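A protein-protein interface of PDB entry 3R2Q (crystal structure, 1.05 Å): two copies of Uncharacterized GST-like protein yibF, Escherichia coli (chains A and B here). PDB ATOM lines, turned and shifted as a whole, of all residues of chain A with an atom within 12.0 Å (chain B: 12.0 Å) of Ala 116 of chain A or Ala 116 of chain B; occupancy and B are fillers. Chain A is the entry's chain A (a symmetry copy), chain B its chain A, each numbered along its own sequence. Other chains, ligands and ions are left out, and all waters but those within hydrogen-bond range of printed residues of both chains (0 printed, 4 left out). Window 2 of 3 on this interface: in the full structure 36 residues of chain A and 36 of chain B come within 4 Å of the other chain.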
ATOM      1  N   ARG A 109      18.243  -2.821  11.611  1.00  0.00           N
ATOM      2  CA  ARG A 109      17.153  -1.913  11.407  1.00  0.00           C
ATOM      3  C   ARG A 109      16.824  -1.753   9.923  1.00  0.00           C
ATOM      4  O   ARG A 109      15.654  -1.639   9.546  1.00  0.00           O
ATOM      5  CB  ARG A 109      17.364  -0.559  12.062  1.00  0.00           C
ATOM      6  CG  ARG A 109      17.485  -0.619  13.574  1.00  0.00           C
ATOM      7  CD  ARG A 109      16.409  -1.380  14.288  1.00  0.00           C
ATOM      8  NE  ARG A 109      15.133  -0.769  13.970  1.00  0.00           N
ATOM      9  CZ  ARG A 109      13.990  -1.446  14.213  1.00  0.00           C
ATOM     10  NH1 ARG A 109      13.979  -2.656  14.750  1.00  0.00           N
ATOM     11  NH2 ARG A 109      12.893  -0.809  13.893  1.00  0.00           N
ATOM     12  N   GLU A 110      17.815  -1.800   9.054  1.00  0.00           N
ATOM     13  CA  GLU A 110      17.603  -1.749   7.613  1.00  0.00           C
ATOM     14  C   GLU A 110      16.740  -2.901   7.189  1.00  0.00           C
ATOM     15  O   GLU A 110      15.799  -2.784   6.425  1.00  0.00           O
ATOM     16  CB  GLU A 110      18.935  -1.735   6.853  1.00  0.00           C
ATOM     17  CG  GLU A 110      18.714  -1.435   5.366  1.00  0.00           C
ATOM     18  CD  GLU A 110      18.328  -0.033   5.043  1.00  0.00           C
ATOM     19  OE1 GLU A 110      18.646   0.913   5.829  1.00  0.00           O
ATOM     20  OE2 GLU A 110      17.723   0.176   4.014  1.00  0.00           O
ATOM     21  N   GLN A 111      17.082  -4.099   7.680  1.00  0.00           N
ATOM     22  CA  GLN A 111      16.380  -5.316   7.324  1.00  0.00           C
ATOM     23  C   GLN A 111      14.977  -5.366   7.947  1.00  0.00           C
ATOM     24  O   GLN A 111      14.191  -6.195   7.478  1.00  0.00           O
ATOM     25  CB  GLN A 111      17.235  -6.507   7.742  1.00  0.00           C
ATOM     26  CG  GLN A 111      18.498  -6.667   6.946  1.00  0.00           C
ATOM     27  CD  GLN A 111      19.464  -7.702   7.477  1.00  0.00           C
ATOM     28  OE1 GLN A 111      19.574  -8.122   8.635  1.00  0.00           O
ATOM     29  NE2 GLN A 111      20.272  -8.172   6.528  1.00  0.00           N
ATOM     30  N   ALA A 112      14.661  -4.529   8.931  1.00  0.00           N
ATOM     31  CA  ALA A 112      13.337  -4.427   9.528  1.00  0.00           C
ATOM     32  C   ALA A 112      12.415  -3.544   8.718  1.00  0.00           C
ATOM     33  O   ALA A 112      11.201  -3.562   8.959  1.00  0.00           O
ATOM     34  CB  ALA A 112      13.401  -3.895  10.969  1.00  0.00           C
ATOM     35  N   ARG A 113      12.933  -2.710   7.813  1.00  0.00           N
ATOM     36  CA  ARG A 113      12.103  -1.825   6.985  1.00  0.00           C
ATOM     37  C   ARG A 113      11.365  -2.664   5.954  1.00  0.00           C
ATOM     38  O   ARG A 113      11.846  -3.751   5.616  1.00  0.00           O
ATOM     39  CB  ARG A 113      12.960  -0.769   6.276  1.00  0.00           C
ATOM     40  CG  ARG A 113      13.716   0.213   7.148  1.00  0.00           C
ATOM     41  CD  ARG A 113      14.892   0.919   6.503  1.00  0.00           C
ATOM     42  NE  ARG A 113      14.585   1.844   5.439  1.00  0.00           N
ATOM     43  CZ  ARG A 113      14.448   3.164   5.627  1.00  0.00           C
ATOM     44  NH1 ARG A 113      14.573   3.806   6.779  1.00  0.00           N
ATOM     45  NH2 ARG A 113      14.172   3.910   4.553  1.00  0.00           N
ATOM     46  N   PRO A 114      10.236  -2.237   5.424  1.00  0.00           N
ATOM     47  CA  PRO A 114       9.544  -2.967   4.349  1.00  0.00           C
ATOM     48  C   PRO A 114      10.527  -3.215   3.210  1.00  0.00           C
ATOM     49  O   PRO A 114      11.435  -2.446   2.955  1.00  0.00           O
ATOM     50  CB  PRO A 114       8.432  -2.047   3.882  1.00  0.00           C
ATOM     51  CG  PRO A 114       8.208  -1.176   5.079  1.00  0.00           C
ATOM     52  CD  PRO A 114       9.556  -1.010   5.737  1.00  0.00           C
ATOM     53  N   ALA A 115      10.325  -4.327   2.505  1.00  0.00           N
ATOM     54  CA  ALA A 115      11.261  -4.825   1.498  1.00  0.00           C
ATOM     55  C   ALA A 115      11.553  -3.750   0.468  1.00  0.00           C
ATOM     56  O   ALA A 115      12.706  -3.473   0.098  1.00  0.00           O
ATOM     57  CB  ALA A 115      10.720  -6.067   0.812  1.00  0.00           C
ATOM     58  N   ALA A 116      10.512  -3.070  -0.006  1.00  0.00           N
ATOM     59  CA  ALA A 116      10.736  -2.116  -1.082  1.00  0.00           C
ATOM     60  C   ALA A 116      11.447  -0.882  -0.577  1.00  0.00           C
ATOM     61  O   ALA A 116      11.809  -0.024  -1.372  1.00  0.00           O
ATOM     62  CB  ALA A 116       9.435  -1.710  -1.731  1.00  0.00           C
ATOM     63  N   GLN A 117      11.639  -0.751   0.747  1.00  0.00           N
ATOM     64  CA  GLN A 117      12.256   0.438   1.313  1.00  0.00           C
ATOM     65  C   GLN A 117      13.730   0.235   1.677  1.00  0.00           C
ATOM     66  O   GLN A 117      14.470   1.128   2.095  1.00  0.00           O
ATOM     67  CB  GLN A 117      11.531   0.940   2.563  1.00  0.00           C
ATOM     68  CG  GLN A 117      10.478   1.976   2.328  1.00  0.00           C
ATOM     69  CD  GLN A 117       9.516   2.271   3.468  1.00  0.00           C
ATOM     70  OE1 GLN A 117       9.873   2.343   4.638  1.00  0.00           O
ATOM     71  NE2 GLN A 117       8.247   2.497   3.162  1.00  0.00           N
ATOM     72  N   GLN A 118      14.165  -1.015   1.507  1.00  0.00           N
ATOM     73  CA  GLN A 118      15.518  -1.389   1.923  1.00  0.00           C
ATOM     74  C   GLN A 118      16.540  -0.966   0.874  1.00  0.00           C
ATOM     75  O   GLN A 118      16.318  -0.956  -0.340  1.00  0.00           O
ATOM     76  CB  GLN A 118      15.546  -2.879   2.155  1.00  0.00           C
ATOM     77  CG  GLN A 118      14.743  -3.355   3.304  1.00  0.00           C
ATOM     78  CD  GLN A 118      14.784  -4.842   3.607  1.00  0.00           C
ATOM     79  OE1 GLN A 118      13.987  -5.350   4.410  1.00  0.00           O
ATOM     80  NE2 GLN A 118      15.683  -5.568   2.943  1.00  0.00           N
ATOM     81  N   SER A 119      17.716  -0.606   1.396  1.00  0.00           N
ATOM     82  CA  SER A 119      18.899  -0.302   0.636  1.00  0.00           C
ATOM     83  C   SER A 119      19.992  -1.387   0.759  1.00  0.00           C
ATOM     84  O   SER A 119      20.625  -1.519   1.832  1.00  0.00           O
ATOM     85  CB  SER A 119      19.484   1.037   1.116  1.00  0.00           C
ATOM     86  OG  SER A 119      20.732   1.275   0.504  1.00  0.00           O
ATOM     87  N   GLU A 120      20.224  -2.136  -0.299  1.00  0.00           N
ATOM     88  CA  GLU A 120      21.295  -3.136  -0.280  1.00  0.00           C
ATOM     89  C   GLU A 120      22.603  -2.392  -0.151  1.00  0.00           C
ATOM     90  O   GLU A 120      23.522  -2.889   0.479  1.00  0.00           O
ATOM     91  CB  GLU A 120      21.242  -4.051  -1.504  1.00  0.00           C
ATOM     92  CG  GLU A 120      22.387  -5.027  -1.612  1.00  0.00           C
ATOM     93  CD  GLU A 120      22.432  -6.194  -0.647  1.00  0.00           C
ATOM     94  OE1 GLU A 120      21.419  -6.510   0.033  1.00  0.00           O
ATOM     95  OE2 GLU A 120      23.492  -6.863  -0.548  1.00  0.00           O
ATOM     96  N   ASP A 121      22.734  -1.184  -0.724  1.00  0.00           N
ATOM     97  CA  ASP A 121      23.981  -0.441  -0.612  1.00  0.00           C
ATOM     98  C   ASP A 121      24.291  -0.142   0.854  1.00  0.00           C
ATOM     99  O   ASP A 121      25.455  -0.256   1.272  1.00  0.00           O
ATOM    100  CB  ASP A 121      23.957   0.818  -1.481  1.00  0.00           C
ATOM    101  CG  ASP A 121      24.032   0.575  -2.983  1.00  0.00           C
ATOM    102  OD1 ASP A 121      24.298  -0.551  -3.473  1.00  0.00           O
ATOM    103  OD2 ASP A 121      23.841   1.531  -3.792  1.00  0.00           O
ATOM    104  N   GLU A 122      23.247   0.246   1.588  1.00  0.00           N
ATOM    105  CA  GLU A 122      23.433   0.504   3.000  1.00  0.00           C
ATOM    106  C   GLU A 122      23.953  -0.721   3.731  1.00  0.00           C
ATOM    107  O   GLU A 122      24.866  -0.649   4.563  1.00  0.00           O
ATOM    108  CB  GLU A 122      22.136   0.939   3.692  1.00  0.00           C
ATOM    109  CG  GLU A 122      22.408   1.535   5.077  1.00  0.00           C
ATOM    110  CD  GLU A 122      23.226   2.803   5.150  1.00  0.00           C
ATOM    111  OE1 GLU A 122      22.812   3.813   4.531  1.00  0.00           O
ATOM    112  OE2 GLU A 122      24.325   2.887   5.756  1.00  0.00           O
ATOM    113  N   LEU A 123      23.352  -1.870   3.459  1.00  0.00           N
ATOM    114  CA  LEU A 123      23.808  -3.125   4.097  1.00  0.00           C
ATOM    115  C   LEU A 123      25.250  -3.435   3.790  1.00  0.00           C
ATOM    116  O   LEU A 123      26.025  -3.851   4.668  1.00  0.00           O
ATOM    117  CB  LEU A 123      22.922  -4.292   3.694  1.00  0.00           C
ATOM    118  CG  LEU A 123      21.538  -4.234   4.269  1.00  0.00           C
ATOM    119  CD1 LEU A 123      20.629  -5.295   3.630  1.00  0.00           C
ATOM    120  CD2 LEU A 123      21.549  -4.408   5.779  1.00  0.00           C
ATOM    121  N   ARG B 109      20.199  11.802   5.952  1.00  0.00           N
ATOM    122  CA  ARG B 109      20.518  10.627   5.196  1.00  0.00           C
ATOM    123  C   ARG B 109      19.258   9.915   4.705  1.00  0.00           C
ATOM    124  O   ARG B 109      19.229   9.383   3.590  1.00  0.00           O
ATOM    125  CB  ARG B 109      21.428   9.663   5.937  1.00  0.00           C
ATOM    126  CG  ARG B 109      22.792  10.239   6.271  1.00  0.00           C
ATOM    127  CD  ARG B 109      23.529  10.881   5.135  1.00  0.00           C
ATOM    128  NE  ARG B 109      23.711   9.890   4.092  1.00  0.00           N
ATOM    129  CZ  ARG B 109      24.048  10.287   2.847  1.00  0.00           C
ATOM    130  NH1 ARG B 109      24.235  11.558   2.529  1.00  0.00           N
ATOM    131  NH2 ARG B 109      24.190   9.318   1.979  1.00  0.00           N
ATOM    132  N   GLU B 110      18.187   9.934   5.474  1.00  0.00           N
ATOM    133  CA  GLU B 110      16.910   9.365   5.064  1.00  0.00           C
ATOM    134  C   GLU B 110      16.431  10.050   3.818  1.00  0.00           C
ATOM    135  O   GLU B 110      15.984   9.452   2.857  1.00  0.00           O
ATOM    136  CB  GLU B 110      15.872   9.453   6.189  1.00  0.00           C
ATOM    137  CG  GLU B 110      14.619   8.641   5.843  1.00  0.00           C
ATOM    138  CD  GLU B 110      14.780   7.161   5.885  1.00  0.00           C
ATOM    139  OE1 GLU B 110      15.680   6.638   6.615  1.00  0.00           O
ATOM    140  OE2 GLU B 110      14.026   6.479   5.225  1.00  0.00           O
ATOM    141  N   GLN B 111      16.490  11.388   3.827  1.00  0.00           N
ATOM    142  CA  GLN B 111      16.017  12.197   2.721  1.00  0.00           C
ATOM    143  C   GLN B 111      16.936  12.079   1.496  1.00  0.00           C
ATOM    144  O   GLN B 111      16.479  12.475   0.419  1.00  0.00           O
ATOM    145  CB  GLN B 111      15.883  13.638   3.199  1.00  0.00           C
ATOM    146  CG  GLN B 111      14.783  13.855   4.198  1.00  0.00           C
ATOM    147  CD  GLN B 111      14.767  15.220   4.848  1.00  0.00           C
ATOM    148  OE1 GLN B 111      15.710  16.005   4.999  1.00  0.00           O
ATOM    149  NE2 GLN B 111      13.557  15.550   5.298  1.00  0.00           N
ATOM    150  N   ALA B 112      18.150  11.554   1.630  1.00  0.00           N
ATOM    151  CA  ALA B 112      19.065  11.310   0.523  1.00  0.00           C
ATOM    152  C   ALA B 112      18.771  10.003  -0.180  1.00  0.00           C
ATOM    153  O   ALA B 112      19.294   9.782  -1.279  1.00  0.00           O
ATOM    154  CB  ALA B 112      20.532  11.309   0.985  1.00  0.00           C
ATOM    155  N   ARG B 113      18.015   9.087   0.429  1.00  0.00           N
ATOM    156  CA  ARG B 113      17.681   7.797  -0.190  1.00  0.00           C
ATOM    157  C   ARG B 113      16.686   8.034  -1.314  1.00  0.00           C
ATOM    158  O   ARG B 113      15.967   9.039  -1.272  1.00  0.00           O
ATOM    159  CB  ARG B 113      17.081   6.831   0.839  1.00  0.00           C
ATOM    160  CG  ARG B 113      17.961   6.418   2.001  1.00  0.00           C
ATOM    161  CD  ARG B 113      17.248   5.873   3.223  1.00  0.00           C
ATOM    162  NE  ARG B 113      16.575   4.607   3.067  1.00  0.00           N
ATOM    163  CZ  ARG B 113      17.128   3.432   3.397  1.00  0.00           C
ATOM    164  NH1 ARG B 113      18.338   3.253   3.906  1.00  0.00           N
ATOM    165  NH2 ARG B 113      16.390   2.333   3.211  1.00  0.00           N
ATOM    166  N   PRO B 114      16.585   7.179  -2.314  1.00  0.00           N
ATOM    167  CA  PRO B 114      15.565   7.315  -3.366  1.00  0.00           C
ATOM    168  C   PRO B 114      14.193   7.428  -2.712  1.00  0.00           C
ATOM    169  O   PRO B 114      13.928   6.882  -1.656  1.00  0.00           O
ATOM    170  CB  PRO B 114      15.648   6.037  -4.180  1.00  0.00           C
ATOM    171  CG  PRO B 114      17.047   5.574  -3.916  1.00  0.00           C
ATOM    172  CD  PRO B 114      17.366   5.988  -2.500  1.00  0.00           C
ATOM    173  N   ALA B 115      13.296   8.157  -3.374  1.00  0.00           N
ATOM    174  CA  ALA B 115      11.993   8.528  -2.823  1.00  0.00           C
ATOM    175  C   ALA B 115      11.240   7.292  -2.366  1.00  0.00           C
ATOM    176  O   ALA B 115      10.679   7.221  -1.261  1.00  0.00           O
ATOM    177  CB  ALA B 115      11.164   9.294  -3.839  1.00  0.00           C
ATOM    178  N   ALA B 116      11.235   6.249  -3.193  1.00  0.00           N
ATOM    179  CA  ALA B 116      10.424   5.091  -2.845  1.00  0.00           C
ATOM    180  C   ALA B 116      11.039   4.318  -1.702  1.00  0.00           C
ATOM    181  O   ALA B 116      10.431   3.374  -1.214  1.00  0.00           O
ATOM    182  CB  ALA B 116      10.251   4.173  -4.031  1.00  0.00           C
ATOM    183  N   GLN B 117      12.260   4.678  -1.269  1.00  0.00           N
ATOM    184  CA  GLN B 117      12.943   3.941  -0.219  1.00  0.00           C
ATOM    185  C   GLN B 117      12.861   4.627   1.148  1.00  0.00           C
ATOM    186  O   GLN B 117      13.299   4.144   2.194  1.00  0.00           O
ATOM    187  CB  GLN B 117      14.421   3.701  -0.532  1.00  0.00           C
ATOM    188  CG  GLN B 117      14.736   2.407  -1.216  1.00  0.00           C
ATOM    189  CD  GLN B 117      16.116   2.258  -1.836  1.00  0.00           C
ATOM    190  OE1 GLN B 117      17.136   2.665  -1.293  1.00  0.00           O
ATOM    191  NE2 GLN B 117      16.207   1.623  -2.995  1.00  0.00           N
ATOM    192  N   GLN B 118      12.268   5.823   1.121  1.00  0.00           N
ATOM    193  CA  GLN B 118      12.220   6.650   2.328  1.00  0.00           C
ATOM    194  C   GLN B 118      11.096   6.192   3.251  1.00  0.00           C
ATOM    195  O   GLN B 118      10.022   5.732   2.853  1.00  0.00           O
ATOM    196  CB  GLN B 118      12.041   8.088   1.909  1.00  0.00           C
ATOM    197  CG  GLN B 118      13.189   8.684   1.188  1.00  0.00           C
ATOM    198  CD  GLN B 118      13.074  10.145   0.793  1.00  0.00           C
ATOM    199  OE1 GLN B 118      13.890  10.659   0.014  1.00  0.00           O
ATOM    200  NE2 GLN B 118      12.041  10.824   1.290  1.00  0.00           N
ATOM    201  N   SER B 119      11.383   6.340   4.547  1.00  0.00           N
ATOM    202  CA  SER B 119      10.458   6.126   5.628  1.00  0.00           C
ATOM    203  C   SER B 119      10.016   7.437   6.315  1.00  0.00           C
ATOM    204  O   SER B 119      10.824   8.070   7.034  1.00  0.00           O
ATOM    205  CB  SER B 119      11.108   5.216   6.684  1.00  0.00           C
ATOM    206  OG  SER B 119      10.287   5.127   7.827  1.00  0.00           O
ATOM    207  N   GLU B 120       8.776   7.836   6.120  1.00  0.00           N
ATOM    208  CA  GLU B 120       8.266   9.031   6.797  1.00  0.00           C
ATOM    209  C   GLU B 120       8.253   8.737   8.279  1.00  0.00           C
ATOM    210  O   GLU B 120       8.480   9.632   9.076  1.00  0.00           O
ATOM    211  CB  GLU B 120       6.899   9.453   6.256  1.00  0.00           C
ATOM    212  CG  GLU B 120       6.257  10.603   6.990  1.00  0.00           C
ATOM    213  CD  GLU B 120       6.841  11.989   6.807  1.00  0.00           C
ATOM    214  OE1 GLU B 120       7.647  12.233   5.870  1.00  0.00           O
ATOM    215  OE2 GLU B 120       6.495  12.905   7.595  1.00  0.00           O
ATOM    216  N   ASP B 121       8.000   7.486   8.702  1.00  0.00           N
ATOM    217  CA  ASP B 121       7.986   7.172  10.122  1.00  0.00           C
ATOM    218  C   ASP B 121       9.353   7.456  10.743  1.00  0.00           C
ATOM    219  O   ASP B 121       9.422   7.999  11.858  1.00  0.00           O
ATOM    220  CB  ASP B 121       7.510   5.740  10.369  1.00  0.00           C
ATOM    221  CG  ASP B 121       6.027   5.493  10.121  1.00  0.00           C
ATOM    222  OD1 ASP B 121       5.211   6.428   9.926  1.00  0.00           O
ATOM    223  OD2 ASP B 121       5.570   4.312  10.124  1.00  0.00           O
ATOM    224  N   GLU B 122      10.400   7.069  10.012  1.00  0.00           N
ATOM    225  CA  GLU B 122      11.737   7.340  10.494  1.00  0.00           C
ATOM    226  C   GLU B 122      11.970   8.827  10.699  1.00  0.00           C
ATOM    227  O   GLU B 122      12.536   9.269  11.706  1.00  0.00           O
ATOM    228  CB  GLU B 122      12.820   6.831   9.536  1.00  0.00           C
ATOM    229  CG  GLU B 122      14.199   6.809  10.204  1.00  0.00           C
ATOM    230  CD  GLU B 122      14.394   5.893  11.389  1.00  0.00           C
ATOM    231  OE1 GLU B 122      14.184   4.666  11.232  1.00  0.00           O
ATOM    232  OE2 GLU B 122      14.705   6.299  12.538  1.00  0.00           O
ATOM    233  N   LEU B 123      11.567   9.627   9.723  1.00  0.00           N
ATOM    234  CA  LEU B 123      11.721  11.094   9.843  1.00  0.00           C
ATOM    235  C   LEU B 123      10.994  11.652  11.038  1.00  0.00           C
ATOM    236  O   LEU B 123      11.509  12.517  11.766  1.00  0.00           O
ATOM    237  CB  LEU B 123      11.263  11.794   8.574  1.00  0.00           C
ATOM    238  CG  LEU B 123      12.160  11.567   7.395  1.00  0.00           C
ATOM    239  CD1 LEU B 123      11.515  12.088   6.101  1.00  0.00           C
ATOM    240  CD2 LEU B 123      13.520  12.218   7.589  1.00  0.00           C
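Of the 15 printed residues of chain B, 6 touch a printed residue of chain A. Among the printed residues, 15 pairs touch across the chains. Among the printed residues, Asp or Glu carboxylates within 4 Å of a Lys or Arg side-chain nitrogen of the other chain: Glu 110 of chain A with Arg 113 of chain B and Arg 113 of chain A with Glu 110 of chain B.
Arg 113 of chain A touches Gln 117 of chain B, and with the chains exchanged Gln 117 of chain A touches Arg 113 of chain B. Arg 113 of chain A touches Ser 119 of chain B, and with the chains exchanged Ser 119 of chain A touches Arg 113 of chain B. Ala 116 of chain B touches its own counterpart, Ala 116 of chain A. Gln 117 of chain A touches Ser 119 of chain B, and with the chains exchanged Ser 119 of chain A touches Gln 117 of chain B. Positions printed for both chains: 109, 110, 111, 112, 113, 114, 115, 116, 117, 118, 119, 120, 121, 122 and 123.
The backbone NH (N) of Ser 119 of chain B lies within hydrogen-bond range of the side-chain carboxylate (OE2) of Glu 110 of chain B, 2.7 Å away. NE of Arg 113 of chain B is in hydrogen-bond range of O of Gln 117 of chain B (3.4 Å). The side-chain carboxylate (OE2) of Glu 110 of chain B is in salt-bridge range of the guanidinium group (NE) of Arg 113 of chain B, 3.8 Å away. The side-chain carboxylate (OE2) of Glu 110 of chain A lies within salt-bridge range of the guanidinium group (NE) of Arg 113 of chain A, 3.8 Å away. The backbone NH (N) of Glu 122 of chain B is in hydrogen-bond range of the side-chain hydroxyl (OG) of Ser 119 of chain B (2.9 Å). O of Arg 113 of chain A sits close to OE1 of Gln 118 of chain A (2.9 Å).
The side-chain carboxylate (OE2) of Glu 110 of chain A lies within salt-bridge range of the guanidinium group (NH2) of Arg 113 of chain B (2.7 Å). O of Gln 117 of chain A is in hydrogen-bond range of NH2 of Arg 113 of chain B (2.5 Å). O of Gln 117 of chain B lies within hydrogen-bond range of NH2 of Arg 113 of chain A, 2.5 Å away. The guanidinium group (NE) of Arg 113 of chain A sits close to the guanidinium group (NH2) of Arg 113 of chain B (2.9 Å). The side-chain carboxylate of Glu 110 of chain B is in salt-bridge range of the guanidinium group of Arg 113 of chain A. The backbone carbonyl oxygen (O) of Gln 117 of chain A sits close to the backbone carbonyl oxygen (O) of Gln 117 of chain B, at 3.2 Å.
Arg 113 of chain A touches Ser 119 of chain B. Ala 116 of chain B touches Ala 116 of chain A. Gln 117 of chain B touches Ala 116 of chain A. CG of Gln 117 of chain A touches O of Ala 116 of chain B (3.8 Å). Gln 117 of chain A touches Gln 118 of chain B. Ser 119 of chain B touches Gln 117 of chain A (CB to OE1, 3.7 Å). Gln 117 of chain B touches Gln 118 of chain A. Ser 119 of chain A touches Arg 113 of chain B (N to NH2, 3.7 Å). OE1 of Gln 117 of chain B touches CB of Ser 119 of chain A, at 3.7 Å.
Printed residues of chain B within 4 Å of Ala 116 of chain A: Ala 116 (3.7 Å) and Gln 117 (3.8 Å). Of the printed residues of chain A, Ala 116 of chain B touches Ala 116 (3.7 Å) and Gln 117 (3.8 Å). No residue of chain B comes within 4 Å of Pro 114 of chain A. No residue of chain B comes within 4 Å of Ala 115 of chain A. No residue of chain A comes within 4 Å of Pro 114 of chain B. Ala 115 of chain B touches none of the printed residues of chain A. Of the printed residues of chain B, Ser 119 of chain A touches Arg 113 and Gln 117. Printed residues of chain A within 4 Å of Gln 117 of chain B: Arg 113 (2.5 Å), Ala 116 (3.8 Å), Gln 117 (3.2 Å), Gln 118 (3.6 Å) and Ser 119 (3.7 Å). The nearest printed residue of chain A that does not touch Ala 116 of chain B is Gln 118 of chain A (6.4 Å). The nearest printed residue of chain A that does not touch Arg 113 of chain B is Gln 118 of chain A (4.03 Å).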
